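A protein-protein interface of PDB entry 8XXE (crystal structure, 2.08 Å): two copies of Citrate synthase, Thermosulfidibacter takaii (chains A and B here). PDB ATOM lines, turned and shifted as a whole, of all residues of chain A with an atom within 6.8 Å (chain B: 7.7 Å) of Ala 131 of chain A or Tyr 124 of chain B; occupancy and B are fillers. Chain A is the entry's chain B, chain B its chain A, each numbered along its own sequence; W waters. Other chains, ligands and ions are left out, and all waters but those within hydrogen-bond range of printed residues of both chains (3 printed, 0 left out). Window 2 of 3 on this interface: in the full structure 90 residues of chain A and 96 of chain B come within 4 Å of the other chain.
Asp 127 of chain A touches Ala 131 of chain B, and with the chains exchanged Ala 131 of chain A touches Asp 127 of chain B. Val 128 of chain A touches Ala 131 of chain B, and with the chains exchanged Ala 131 of chain A touches Val 128 of chain B. Val 128 of chain A touches Met 132 of chain B, and with the chains exchanged Met 132 of chain A touches Val 128 of chain B.
Printed residues of chain A that touch a printed residue of chain B: Asp 127, Val 128, Ala 131, Met 132 and Pro 133. Hydrophobic or aromatic side chains of chain A within 4 Å of the printed part of chain B: Val 128, Ala 131, Met 132 and Pro 133. Printed residues of chain B that touch a printed residue of chain A: Tyr 124, Asp 127, Val 128, Ala 131, Met 132 and Arg 151. Hydrophobic or aromatic side chains of chain B within 4 Å of the printed part of chain A: Tyr 124, Val 128, Ala 131 and Met 132.
Asp 127 of chain A touches Ala 131 of chain B (O to CB, 3.8 Å). Val 128 of chain A touches Ala 131 of chain B. Val 128 of chain A touches Met 132 of chain B (CG2 to CG, 3.8 Å). Tyr 124 of chain B touches Ala 131 of chain A. CB of Ala 131 of chain A touches O of Asp 127 of chain B, at 3.8 Å. Ala 131 of chain A touches Val 128 of chain B. Val 128 of chain B touches Met 132 of chain A. Pro 133 of chain A touches Tyr 124 of chain B. Pro 133 of chain A touches Arg 151 of chain B (CB to NE, 3.7 Å).
Water W2 bridges O of Ala 131 of chain B (2.6 Å) and OD2 of Asp 127 of chain A (2.6 Å). Water W1 bridges the backbone carbonyl oxygen of Ala 131 of chain A and the side-chain carboxylate of Asp 127 of chain B. Water W3 lies within hydrogen-bond range of O of Ala 148 of chain B and OG1 of Thr 136 of chain A.
Ala 131 of chain A touches three residues of chain B. Of chain A, only Ala 131 (3.8 Å) and Pro 133 (3.5 Å) come within 4 Å of Tyr 124 of chain B. Of the printed residues of chain B, Met 132 of chain A touches Val 128 (3.8 Å). Printed residues of chain A within 4 Å of Arg 151 of chain B: Pro 133 (3.7 Å). Val 134 of chain A touches none of the printed residues of chain B. Phe 126 of chain A touches none of the printed residues of chain B. The nearest residue of chain B that does not touch Ala 131 of chain A is Ala 131 of chain B (4.5 Å). The nearest printed residue of chain A that does not touch Ala 131 of chain B is Ala 131 of chain A (4.5 Å).
OD1 of Asp 127 of chain B sits at hydrogen-bond distance from NE2 of Gln 123 of chain B (3.2 Å). OE1 of Glu 152 of chain B sits at hydrogen-bond distance from OH of Tyr 124 of chain B. NH1 of Arg 151 of chain B lies within salt-bridge range of OE1 of Glu 152 of chain B. The guanidinium group (NH1) of Arg 193 of chain A lies within hydrogen-bond range of the backbone carbonyl oxygen (O) of Met 132 of chain A (2.8 Å). OG1 of Thr 136 of chain A sits at hydrogen-bond distance from O of Pro 133 of chain A (2.7 Å).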
ATOM      1  N   PHE A 126     -38.467 -31.672 -18.646  1.00  0.00           N
ATOM      2  CA  PHE A 126     -38.511 -30.493 -17.801  1.00  0.00           C
ATOM      3  C   PHE A 126     -37.309 -30.427 -16.861  1.00  0.00           C
ATOM      4  O   PHE A 126     -36.894 -29.330 -16.538  1.00  0.00           O
ATOM      5  CB  PHE A 126     -39.806 -30.440 -16.994  1.00  0.00           C
ATOM      6  CG  PHE A 126     -41.005 -30.463 -17.895  1.00  0.00           C
ATOM      7  CD1 PHE A 126     -41.367 -29.338 -18.625  1.00  0.00           C
ATOM      8  CD2 PHE A 126     -41.738 -31.628 -18.054  1.00  0.00           C
ATOM      9  CE1 PHE A 126     -42.466 -29.371 -19.473  1.00  0.00           C
ATOM     10  CE2 PHE A 126     -42.847 -31.656 -18.877  1.00  0.00           C
ATOM     11  CZ  PHE A 126     -43.211 -30.528 -19.587  1.00  0.00           C
ATOM     12  N   ASP A 127     -36.802 -31.564 -16.383  1.00  0.00           N
ATOM     13  CA  ASP A 127     -35.575 -31.557 -15.591  1.00  0.00           C
ATOM     14  C   ASP A 127     -34.443 -30.970 -16.435  1.00  0.00           C
ATOM     15  O   ASP A 127     -33.601 -30.249 -15.933  1.00  0.00           O
ATOM     16  CB  ASP A 127     -35.160 -32.952 -15.119  1.00  0.00           C
ATOM     17  CG  ASP A 127     -36.174 -33.650 -14.204  1.00  0.00           C
ATOM     18  OD1 ASP A 127     -37.094 -32.971 -13.711  1.00  0.00           O
ATOM     19  OD2 ASP A 127     -36.067 -34.877 -14.033  1.00  0.00           O
ATOM     20  N   VAL A 128     -34.358 -31.367 -17.695  1.00  0.00           N
ATOM     21  CA  VAL A 128     -33.304 -30.872 -18.562  1.00  0.00           C
ATOM     22  C   VAL A 128     -33.442 -29.370 -18.701  1.00  0.00           C
ATOM     23  O   VAL A 128     -32.461 -28.650 -18.516  1.00  0.00           O
ATOM     24  CB  VAL A 128     -33.313 -31.574 -19.936  1.00  0.00           C
ATOM     25  CG1 VAL A 128     -32.506 -30.836 -20.969  1.00  0.00           C
ATOM     26  CG2 VAL A 128     -32.794 -33.006 -19.839  1.00  0.00           C
ATOM     27  N   LEU A 129     -34.661 -28.916 -18.993  1.00  0.00           N
ATOM     28  CA  LEU A 129     -34.931 -27.509 -19.197  1.00  0.00           C
ATOM     29  C   LEU A 129     -34.550 -26.738 -17.943  1.00  0.00           C
ATOM     30  O   LEU A 129     -33.918 -25.676 -18.047  1.00  0.00           O
ATOM     31  CB  LEU A 129     -36.405 -27.294 -19.561  1.00  0.00           C
ATOM     32  CG  LEU A 129     -36.804 -27.684 -20.981  1.00  0.00           C
ATOM     33  CD1 LEU A 129     -38.309 -27.656 -21.126  1.00  0.00           C
ATOM     34  CD2 LEU A 129     -36.163 -26.742 -21.990  1.00  0.00           C
ATOM     35  N   ARG A 130     -34.882 -27.270 -16.758  1.00  0.00           N
ATOM     36  CA  ARG A 130     -34.627 -26.516 -15.535  1.00  0.00           C
ATOM     37  C   ARG A 130     -33.141 -26.539 -15.182  1.00  0.00           C
ATOM     38  O   ARG A 130     -32.673 -25.658 -14.509  1.00  0.00           O
ATOM     39  CB  ARG A 130     -35.383 -27.015 -14.300  1.00  0.00           C
ATOM     40  CG  ARG A 130     -36.841 -26.606 -14.195  1.00  0.00           C
ATOM     41  CD  ARG A 130     -37.452 -26.965 -12.836  1.00  0.00           C
ATOM     42  NE  ARG A 130     -37.297 -25.897 -11.864  1.00  0.00           N
ATOM     43  CZ  ARG A 130     -37.867 -24.699 -11.966  1.00  0.00           C
ATOM     44  NH1 ARG A 130     -37.707 -23.793 -11.016  1.00  0.00           N
ATOM     45  NH2 ARG A 130     -38.628 -24.412 -13.006  1.00  0.00           N
ATOM     46  N   ALA A 131     -32.361 -27.491 -15.677  1.00  0.00           N
ATOM     47  CA  ALA A 131     -30.929 -27.515 -15.360  1.00  0.00           C
ATOM     48  C   ALA A 131     -30.165 -26.452 -16.168  1.00  0.00           C
ATOM     49  O   ALA A 131     -29.028 -26.106 -15.861  1.00  0.00           O
ATOM     50  CB  ALA A 131     -30.406 -28.904 -15.676  1.00  0.00           C
ATOM     51  N   MET A 132     -30.759 -25.984 -17.264  1.00  0.00           N
ATOM     52  CA  MET A 132     -30.155 -24.910 -18.036  1.00  0.00           C
ATOM     53  C   MET A 132     -30.344 -23.595 -17.295  1.00  0.00           C
ATOM     54  O   MET A 132     -31.428 -23.311 -16.795  1.00  0.00           O
ATOM     55  CB  MET A 132     -30.816 -24.801 -19.399  1.00  0.00           C
ATOM     56  CG  MET A 132     -30.511 -26.021 -20.202  1.00  0.00           C
ATOM     57  SD  MET A 132     -31.408 -26.027 -21.766  1.00  0.00           S
ATOM     58  CE  MET A 132     -30.034 -25.620 -22.823  1.00  0.00           C
ATOM     59  N   PRO A 133     -29.307 -22.745 -17.226  1.00  0.00           N
ATOM     60  CA  PRO A 133     -29.447 -21.441 -16.583  1.00  0.00           C
ATOM     61  C   PRO A 133     -30.530 -20.625 -17.271  1.00  0.00           C
ATOM     62  O   PRO A 133     -30.660 -20.668 -18.487  1.00  0.00           O
ATOM     63  CB  PRO A 133     -28.067 -20.796 -16.739  1.00  0.00           C
ATOM     64  CG  PRO A 133     -27.128 -21.961 -16.990  1.00  0.00           C
ATOM     65  CD  PRO A 133     -27.941 -23.011 -17.721  1.00  0.00           C
ATOM     66  N   VAL A 134     -31.310 -19.905 -16.469  1.00  0.00           N
ATOM     67  CA  VAL A 134     -32.521 -19.289 -16.955  1.00  0.00           C
ATOM     68  C   VAL A 134     -32.201 -18.194 -17.988  1.00  0.00           C
ATOM     69  O   VAL A 134     -33.059 -17.867 -18.807  1.00  0.00           O
ATOM     70  CB  VAL A 134     -33.361 -18.800 -15.777  1.00  0.00           C
ATOM     71  CG1 VAL A 134     -32.741 -17.585 -15.082  1.00  0.00           C
ATOM     72  CG2 VAL A 134     -34.815 -18.536 -16.219  1.00  0.00           C
ATOM     73  N   THR A 136     -30.167 -18.551 -20.407  1.00  0.00           N
ATOM     74  CA  THR A 136     -29.857 -19.184 -21.679  1.00  0.00           C
ATOM     75  C   THR A 136     -30.873 -18.728 -22.720  1.00  0.00           C
ATOM     76  O   THR A 136     -32.073 -18.626 -22.443  1.00  0.00           O
ATOM     77  CB  THR A 136     -29.912 -20.709 -21.562  1.00  0.00           C
ATOM     78  OG1 THR A 136     -28.990 -21.118 -20.554  1.00  0.00           O
ATOM     79  CG2 THR A 136     -29.619 -21.418 -22.857  1.00  0.00           C
ATOM     80  N   ARG A 193     -40.953 -19.836 -17.555  1.00  0.00           N
ATOM     81  CA  ARG A 193     -39.796 -19.817 -16.677  1.00  0.00           C
ATOM     82  C   ARG A 193     -38.974 -18.540 -16.869  1.00  0.00           C
ATOM     83  O   ARG A 193     -38.542 -17.936 -15.896  1.00  0.00           O
ATOM     84  CB  ARG A 193     -38.912 -21.049 -16.883  1.00  0.00           C
ATOM     85  CG  ARG A 193     -37.767 -21.104 -15.875  1.00  0.00           C
ATOM     86  CD  ARG A 193     -36.804 -22.235 -16.080  1.00  0.00           C
ATOM     87  NE  ARG A 193     -35.747 -22.251 -15.059  1.00  0.00           N
ATOM     88  CZ  ARG A 193     -34.487 -22.507 -15.361  1.00  0.00           C
ATOM     89  NH1 ARG A 193     -34.199 -22.830 -16.601  1.00  0.00           N
ATOM     90  NH2 ARG A 193     -33.544 -22.472 -14.442  1.00  0.00           N
ATOM     91  N   VAL B 121     -15.280 -26.250 -18.026  1.00  0.00           N
ATOM     92  CA  VAL B 121     -16.585 -26.721 -18.449  1.00  0.00           C
ATOM     93  C   VAL B 121     -17.577 -26.295 -17.376  1.00  0.00           C
ATOM     94  O   VAL B 121     -17.393 -26.633 -16.227  1.00  0.00           O
ATOM     95  CB  VAL B 121     -16.606 -28.237 -18.717  1.00  0.00           C
ATOM     96  CG1 VAL B 121     -17.994 -28.713 -19.095  1.00  0.00           C
ATOM     97  CG2 VAL B 121     -15.585 -28.617 -19.782  1.00  0.00           C
ATOM     98  N   PRO B 122     -18.633 -25.509 -17.696  1.00  0.00           N
ATOM     99  CA  PRO B 122     -19.568 -25.062 -16.668  1.00  0.00           C
ATOM    100  C   PRO B 122     -20.198 -26.194 -15.860  1.00  0.00           C
ATOM    101  O   PRO B 122     -20.533 -27.240 -16.381  1.00  0.00           O
ATOM    102  CB  PRO B 122     -20.647 -24.341 -17.483  1.00  0.00           C
ATOM    103  CG  PRO B 122     -19.915 -23.881 -18.743  1.00  0.00           C
ATOM    104  CD  PRO B 122     -19.011 -25.055 -19.046  1.00  0.00           C
ATOM    105  N   GLN B 123     -20.441 -25.946 -14.573  1.00  0.00           N
ATOM    106  CA  GLN B 123     -21.133 -26.895 -13.751  1.00  0.00           C
ATOM    107  C   GLN B 123     -22.520 -27.227 -14.332  1.00  0.00           C
ATOM    108  O   GLN B 123     -22.954 -28.356 -14.220  1.00  0.00           O
ATOM    109  CB  GLN B 123     -21.164 -26.373 -12.325  1.00  0.00           C
ATOM    110  CG  GLN B 123     -21.971 -27.248 -11.407  1.00  0.00           C
ATOM    111  CD  GLN B 123     -21.367 -28.618 -11.310  1.00  0.00           C
ATOM    112  OE1 GLN B 123     -20.168 -28.759 -11.091  1.00  0.00           O
ATOM    113  NE2 GLN B 123     -22.192 -29.636 -11.536  1.00  0.00           N
ATOM    114  N   TYR B 124     -23.203 -26.302 -14.990  1.00  0.00           N
ATOM    115  CA  TYR B 124     -24.565 -26.563 -15.431  1.00  0.00           C
ATOM    116  C   TYR B 124     -24.588 -27.548 -16.599  1.00  0.00           C
ATOM    117  O   TYR B 124     -25.608 -28.157 -16.838  1.00  0.00           O
ATOM    118  CB  TYR B 124     -25.308 -25.261 -15.747  1.00  0.00           C
ATOM    119  CG  TYR B 124     -24.737 -24.488 -16.903  1.00  0.00           C
ATOM    120  CD1 TYR B 124     -24.949 -24.919 -18.209  1.00  0.00           C
ATOM    121  CD2 TYR B 124     -23.945 -23.376 -16.703  1.00  0.00           C
ATOM    122  CE1 TYR B 124     -24.378 -24.268 -19.285  1.00  0.00           C
ATOM    123  CE2 TYR B 124     -23.435 -22.661 -17.781  1.00  0.00           C
ATOM    124  CZ  TYR B 124     -23.638 -23.119 -19.070  1.00  0.00           C
ATOM    125  OH  TYR B 124     -23.069 -22.477 -20.141  1.00  0.00           O
ATOM    126  N   VAL B 125     -23.491 -27.685 -17.348  1.00  0.00           N
ATOM    127  CA  VAL B 125     -23.388 -28.686 -18.411  1.00  0.00           C
ATOM    128  C   VAL B 125     -23.494 -30.085 -17.805  1.00  0.00           C
ATOM    129  O   VAL B 125     -24.239 -30.914 -18.296  1.00  0.00           O
ATOM    130  CB  VAL B 125     -22.082 -28.539 -19.213  1.00  0.00           C
ATOM    131  CG1 VAL B 125     -21.802 -29.753 -20.066  1.00  0.00           C
ATOM    132  CG2 VAL B 125     -22.076 -27.305 -20.079  1.00  0.00           C
ATOM    133  N   PHE B 126     -22.843 -30.308 -16.658  1.00  0.00           N
ATOM    134  CA  PHE B 126     -22.973 -31.572 -15.943  1.00  0.00           C
ATOM    135  C   PHE B 126     -24.373 -31.768 -15.366  1.00  0.00           C
ATOM    136  O   PHE B 126     -24.870 -32.902 -15.335  1.00  0.00           O
ATOM    137  CB  PHE B 126     -21.911 -31.663 -14.847  1.00  0.00           C
ATOM    138  CG  PHE B 126     -20.517 -31.591 -15.410  1.00  0.00           C
ATOM    139  CD1 PHE B 126     -20.000 -32.658 -16.135  1.00  0.00           C
ATOM    140  CD2 PHE B 126     -19.736 -30.450 -15.244  1.00  0.00           C
ATOM    141  CE1 PHE B 126     -18.709 -32.596 -16.650  1.00  0.00           C
ATOM    142  CE2 PHE B 126     -18.467 -30.373 -15.798  1.00  0.00           C
ATOM    143  CZ  PHE B 126     -17.959 -31.444 -16.502  1.00  0.00           C
ATOM    144  N   ASP B 127     -24.982 -30.701 -14.833  1.00  0.00           N
ATOM    145  CA  ASP B 127     -26.381 -30.785 -14.408  1.00  0.00           C
ATOM    146  C   ASP B 127     -27.295 -31.202 -15.573  1.00  0.00           C
ATOM    147  O   ASP B 127     -28.231 -31.993 -15.412  1.00  0.00           O
ATOM    148  CB  ASP B 127     -26.880 -29.448 -13.855  1.00  0.00           C
ATOM    149  CG  ASP B 127     -26.116 -28.884 -12.650  1.00  0.00           C
ATOM    150  OD1 ASP B 127     -25.348 -29.639 -12.037  1.00  0.00           O
ATOM    151  OD2 ASP B 127     -26.299 -27.658 -12.334  1.00  0.00           O
ATOM    152  N   VAL B 128     -27.082 -30.625 -16.761  1.00  0.00           N
ATOM    153  CA  VAL B 128     -27.857 -31.026 -17.926  1.00  0.00           C
ATOM    154  C   VAL B 128     -27.637 -32.503 -18.223  1.00  0.00           C
ATOM    155  O   VAL B 128     -28.609 -33.245 -18.416  1.00  0.00           O
ATOM    156  CB  VAL B 128     -27.593 -30.134 -19.153  1.00  0.00           C
ATOM    157  CG1 VAL B 128     -28.201 -30.700 -20.412  1.00  0.00           C
ATOM    158  CG2 VAL B 128     -28.142 -28.751 -18.903  1.00  0.00           C
ATOM    159  N   LEU B 129     -26.378 -32.953 -18.206  1.00  0.00           N
ATOM    160  CA  LEU B 129     -26.102 -34.344 -18.505  1.00  0.00           C
ATOM    161  C   LEU B 129     -26.760 -35.254 -17.463  1.00  0.00           C
ATOM    162  O   LEU B 129     -27.291 -36.291 -17.835  1.00  0.00           O
ATOM    163  CB  LEU B 129     -24.596 -34.573 -18.558  1.00  0.00           C
ATOM    164  CG  LEU B 129     -23.887 -33.959 -19.762  1.00  0.00           C
ATOM    165  CD1 LEU B 129     -22.406 -33.937 -19.515  1.00  0.00           C
ATOM    166  CD2 LEU B 129     -24.206 -34.716 -21.043  1.00  0.00           C
ATOM    167  N   ARG B 130     -26.727 -34.896 -16.168  1.00  0.00           N
ATOM    168  CA  ARG B 130     -27.272 -35.777 -15.154  1.00  0.00           C
ATOM    169  C   ARG B 130     -28.793 -35.782 -15.190  1.00  0.00           C
ATOM    170  O   ARG B 130     -29.400 -36.756 -14.792  1.00  0.00           O
ATOM    171  CB  ARG B 130     -26.820 -35.455 -13.728  1.00  0.00           C
ATOM    172  CG  ARG B 130     -25.371 -35.789 -13.427  1.00  0.00           C
ATOM    173  CD  ARG B 130     -25.031 -35.662 -11.938  1.00  0.00           C
ATOM    174  NE  ARG B 130     -25.449 -36.843 -11.221  1.00  0.00           N
ATOM    175  CZ  ARG B 130     -24.834 -38.021 -11.283  1.00  0.00           C
ATOM    176  NH1 ARG B 130     -25.236 -39.000 -10.489  1.00  0.00           N
ATOM    177  NH2 ARG B 130     -23.793 -38.206 -12.091  1.00  0.00           N
ATOM    178  N   ALA B 131     -29.424 -34.739 -15.728  1.00  0.00           N
ATOM    179  CA  ALA B 131     -30.890 -34.708 -15.793  1.00  0.00           C
ATOM    180  C   ALA B 131     -31.442 -35.616 -16.897  1.00  0.00           C
ATOM    181  O   ALA B 131     -32.613 -35.971 -16.850  1.00  0.00           O
ATOM    182  CB  ALA B 131     -31.362 -33.287 -16.027  1.00  0.00           C
ATOM    183  N   MET B 132     -30.613 -35.983 -17.878  1.00  0.00           N
ATOM    184  CA  MET B 132     -31.003 -36.919 -18.921  1.00  0.00           C
ATOM    185  C   MET B 132     -30.967 -38.330 -18.339  1.00  0.00           C
ATOM    186  O   MET B 132     -30.041 -38.699 -17.626  1.00  0.00           O
ATOM    187  CB  MET B 132     -30.061 -36.844 -20.126  1.00  0.00           C
ATOM    188  CG  MET B 132     -30.021 -35.444 -20.721  1.00  0.00           C
ATOM    189  SD  MET B 132     -28.864 -35.358 -22.111  1.00  0.00           S
ATOM    190  CE  MET B 132     -30.083 -35.676 -23.369  1.00  0.00           C
ATOM    191  N   GLY B 145     -25.064 -31.858 -24.273  1.00  0.00           N
ATOM    192  CA  GLY B 145     -24.106 -31.179 -23.419  1.00  0.00           C
ATOM    193  C   GLY B 145     -23.381 -30.068 -24.167  1.00  0.00           C
ATOM    194  O   GLY B 145     -23.097 -29.022 -23.603  1.00  0.00           O
ATOM    195  N   ILE B 146     -23.018 -30.342 -25.415  1.00  0.00           N
ATOM    196  CA  ILE B 146     -22.398 -29.349 -26.281  1.00  0.00           C
ATOM    197  C   ILE B 146     -23.357 -28.184 -26.476  1.00  0.00           C
ATOM    198  O   ILE B 146     -22.969 -27.023 -26.305  1.00  0.00           O
ATOM    199  CB  ILE B 146     -22.008 -29.953 -27.647  1.00  0.00           C
ATOM    200  CG1 ILE B 146     -20.944 -31.036 -27.514  1.00  0.00           C
ATOM    201  CG2 ILE B 146     -21.569 -28.844 -28.599  1.00  0.00           C
ATOM    202  CD1 ILE B 146     -20.788 -31.868 -28.761  1.00  0.00           C
ATOM    203  N   LEU B 147     -24.617 -28.487 -26.844  1.00  0.00           N
ATOM    204  CA  LEU B 147     -25.583 -27.413 -27.027  1.00  0.00           C
ATOM    205  C   LEU B 147     -25.768 -26.577 -25.751  1.00  0.00           C
ATOM    206  O   LEU B 147     -25.891 -25.372 -25.815  1.00  0.00           O
ATOM    207  CB  LEU B 147     -26.886 -28.031 -27.504  1.00  0.00           C
ATOM    208  CG  LEU B 147     -28.034 -27.059 -27.715  1.00  0.00           C
ATOM    209  CD1 LEU B 147     -27.654 -25.981 -28.708  1.00  0.00           C
ATOM    210  CD2 LEU B 147     -29.267 -27.806 -28.174  1.00  0.00           C
ATOM    211  N   ALA B 148     -25.807 -27.180 -24.559  1.00  0.00           N
ATOM    212  CA  ALA B 148     -26.030 -26.388 -23.347  1.00  0.00           C
ATOM    213  C   ALA B 148     -24.948 -25.326 -23.131  1.00  0.00           C
ATOM    214  O   ALA B 148     -25.179 -24.252 -22.565  1.00  0.00           O
ATOM    215  CB  ALA B 148     -26.091 -27.299 -22.155  1.00  0.00           C
ATOM    216  N   MET B 149     -23.747 -25.600 -23.632  1.00  0.00           N
ATOM    217  CA  MET B 149     -22.623 -24.737 -23.389  1.00  0.00           C
ATOM    218  C   MET B 149     -22.649 -23.564 -24.366  1.00  0.00           C
ATOM    219  O   MET B 149     -21.793 -22.686 -24.308  1.00  0.00           O
ATOM    220  CB  MET B 149     -21.357 -25.592 -23.490  1.00  0.00           C
ATOM    221  CG  MET B 149     -20.090 -24.931 -22.965  1.00  0.00           C
ATOM    222  SD  MET B 149     -18.760 -26.193 -22.892  1.00  0.00           S
ATOM    223  CE  MET B 149     -17.404 -25.050 -22.623  1.00  0.00           C
ATOM    224  N   GLN B 150     -23.717 -23.461 -25.174  1.00  0.00           N
ATOM    225  CA  GLN B 150     -23.882 -22.361 -26.107  1.00  0.00           C
ATOM    226  C   GLN B 150     -24.027 -21.053 -25.340  1.00  0.00           C
ATOM    227  O   GLN B 150     -23.695 -20.000 -25.859  1.00  0.00           O
ATOM    228  CB  GLN B 150     -25.080 -22.596 -27.019  1.00  0.00           C
ATOM    229  CG  GLN B 150     -25.356 -21.496 -28.045  1.00  0.00           C
ATOM    230  CD  GLN B 150     -26.074 -20.255 -27.561  1.00  0.00           C
ATOM    231  OE1 GLN B 150     -26.855 -20.224 -26.604  1.00  0.00           O
ATOM    232  NE2 GLN B 150     -25.794 -19.168 -28.256  1.00  0.00           N
ATOM    233  N   ARG B 151     -24.473 -21.113 -24.080  1.00  0.00           N
ATOM    234  CA  ARG B 151     -24.548 -19.909 -23.263  1.00  0.00           C
ATOM    235  C   ARG B 151     -23.187 -19.203 -23.109  1.00  0.00           C
ATOM    236  O   ARG B 151     -23.162 -18.016 -22.842  1.00  0.00           O
ATOM    237  CB  ARG B 151     -25.110 -20.298 -21.887  1.00  0.00           C
ATOM    238  CG  ARG B 151     -25.173 -19.148 -20.887  1.00  0.00           C
ATOM    239  CD  ARG B 151     -25.329 -19.695 -19.490  1.00  0.00           C
ATOM    240  NE  ARG B 151     -25.577 -18.669 -18.480  1.00  0.00           N
ATOM    241  CZ  ARG B 151     -24.645 -18.169 -17.677  1.00  0.00           C
ATOM    242  NH1 ARG B 151     -23.377 -18.551 -17.791  1.00  0.00           N
ATOM    243  NH2 ARG B 151     -24.982 -17.228 -16.815  1.00  0.00           N
ATOM    244  N   GLU B 152     -22.057 -19.924 -23.222  1.00  0.00           N
ATOM    245  CA  GLU B 152     -20.729 -19.337 -23.079  1.00  0.00           C
ATOM    246  C   GLU B 152     -20.163 -18.860 -24.427  1.00  0.00           C
ATOM    247  O   GLU B 152     -18.978 -18.562 -24.519  1.00  0.00           O
ATOM    248  CB  GLU B 152     -19.762 -20.377 -22.486  1.00  0.00           C
ATOM    249  CG  GLU B 152     -20.244 -21.014 -21.170  1.00  0.00           C
ATOM    250  CD  GLU B 152     -20.901 -20.057 -20.170  1.00  0.00           C
ATOM    251  OE1 GLU B 152     -21.951 -20.405 -19.599  1.00  0.00           O
ATOM    252  OE2 GLU B 152     -20.389 -18.940 -19.980  1.00  0.00           O
ATOM    253  N   SER B 153     -20.978 -18.807 -25.492  1.00  0.00           N
ATOM    254  CA  SER B 153     -20.470 -18.467 -26.818  1.00  0.00           C
ATOM    255  C   SER B 153     -20.018 -16.999 -26.870  1.00  0.00           C
ATOM    256  O   SER B 153     -20.814 -16.108 -26.659  1.00  0.00           O
ATOM    257  CB  SER B 153     -21.474 -18.723 -27.896  1.00  0.00           C
ATOM    258  OG  SER B 153     -20.955 -18.294 -29.156  1.00  0.00           O
HETATM  259  O   HOH W   1     -28.074 -26.017 -13.410  1.00  0.00           O
HETATM  260  O   HOH W   2     -34.094 -36.357 -14.797  1.00  0.00           O
HETATM  261  O   HOH W   3     -27.651 -23.748 -21.176  1.00  0.00           O
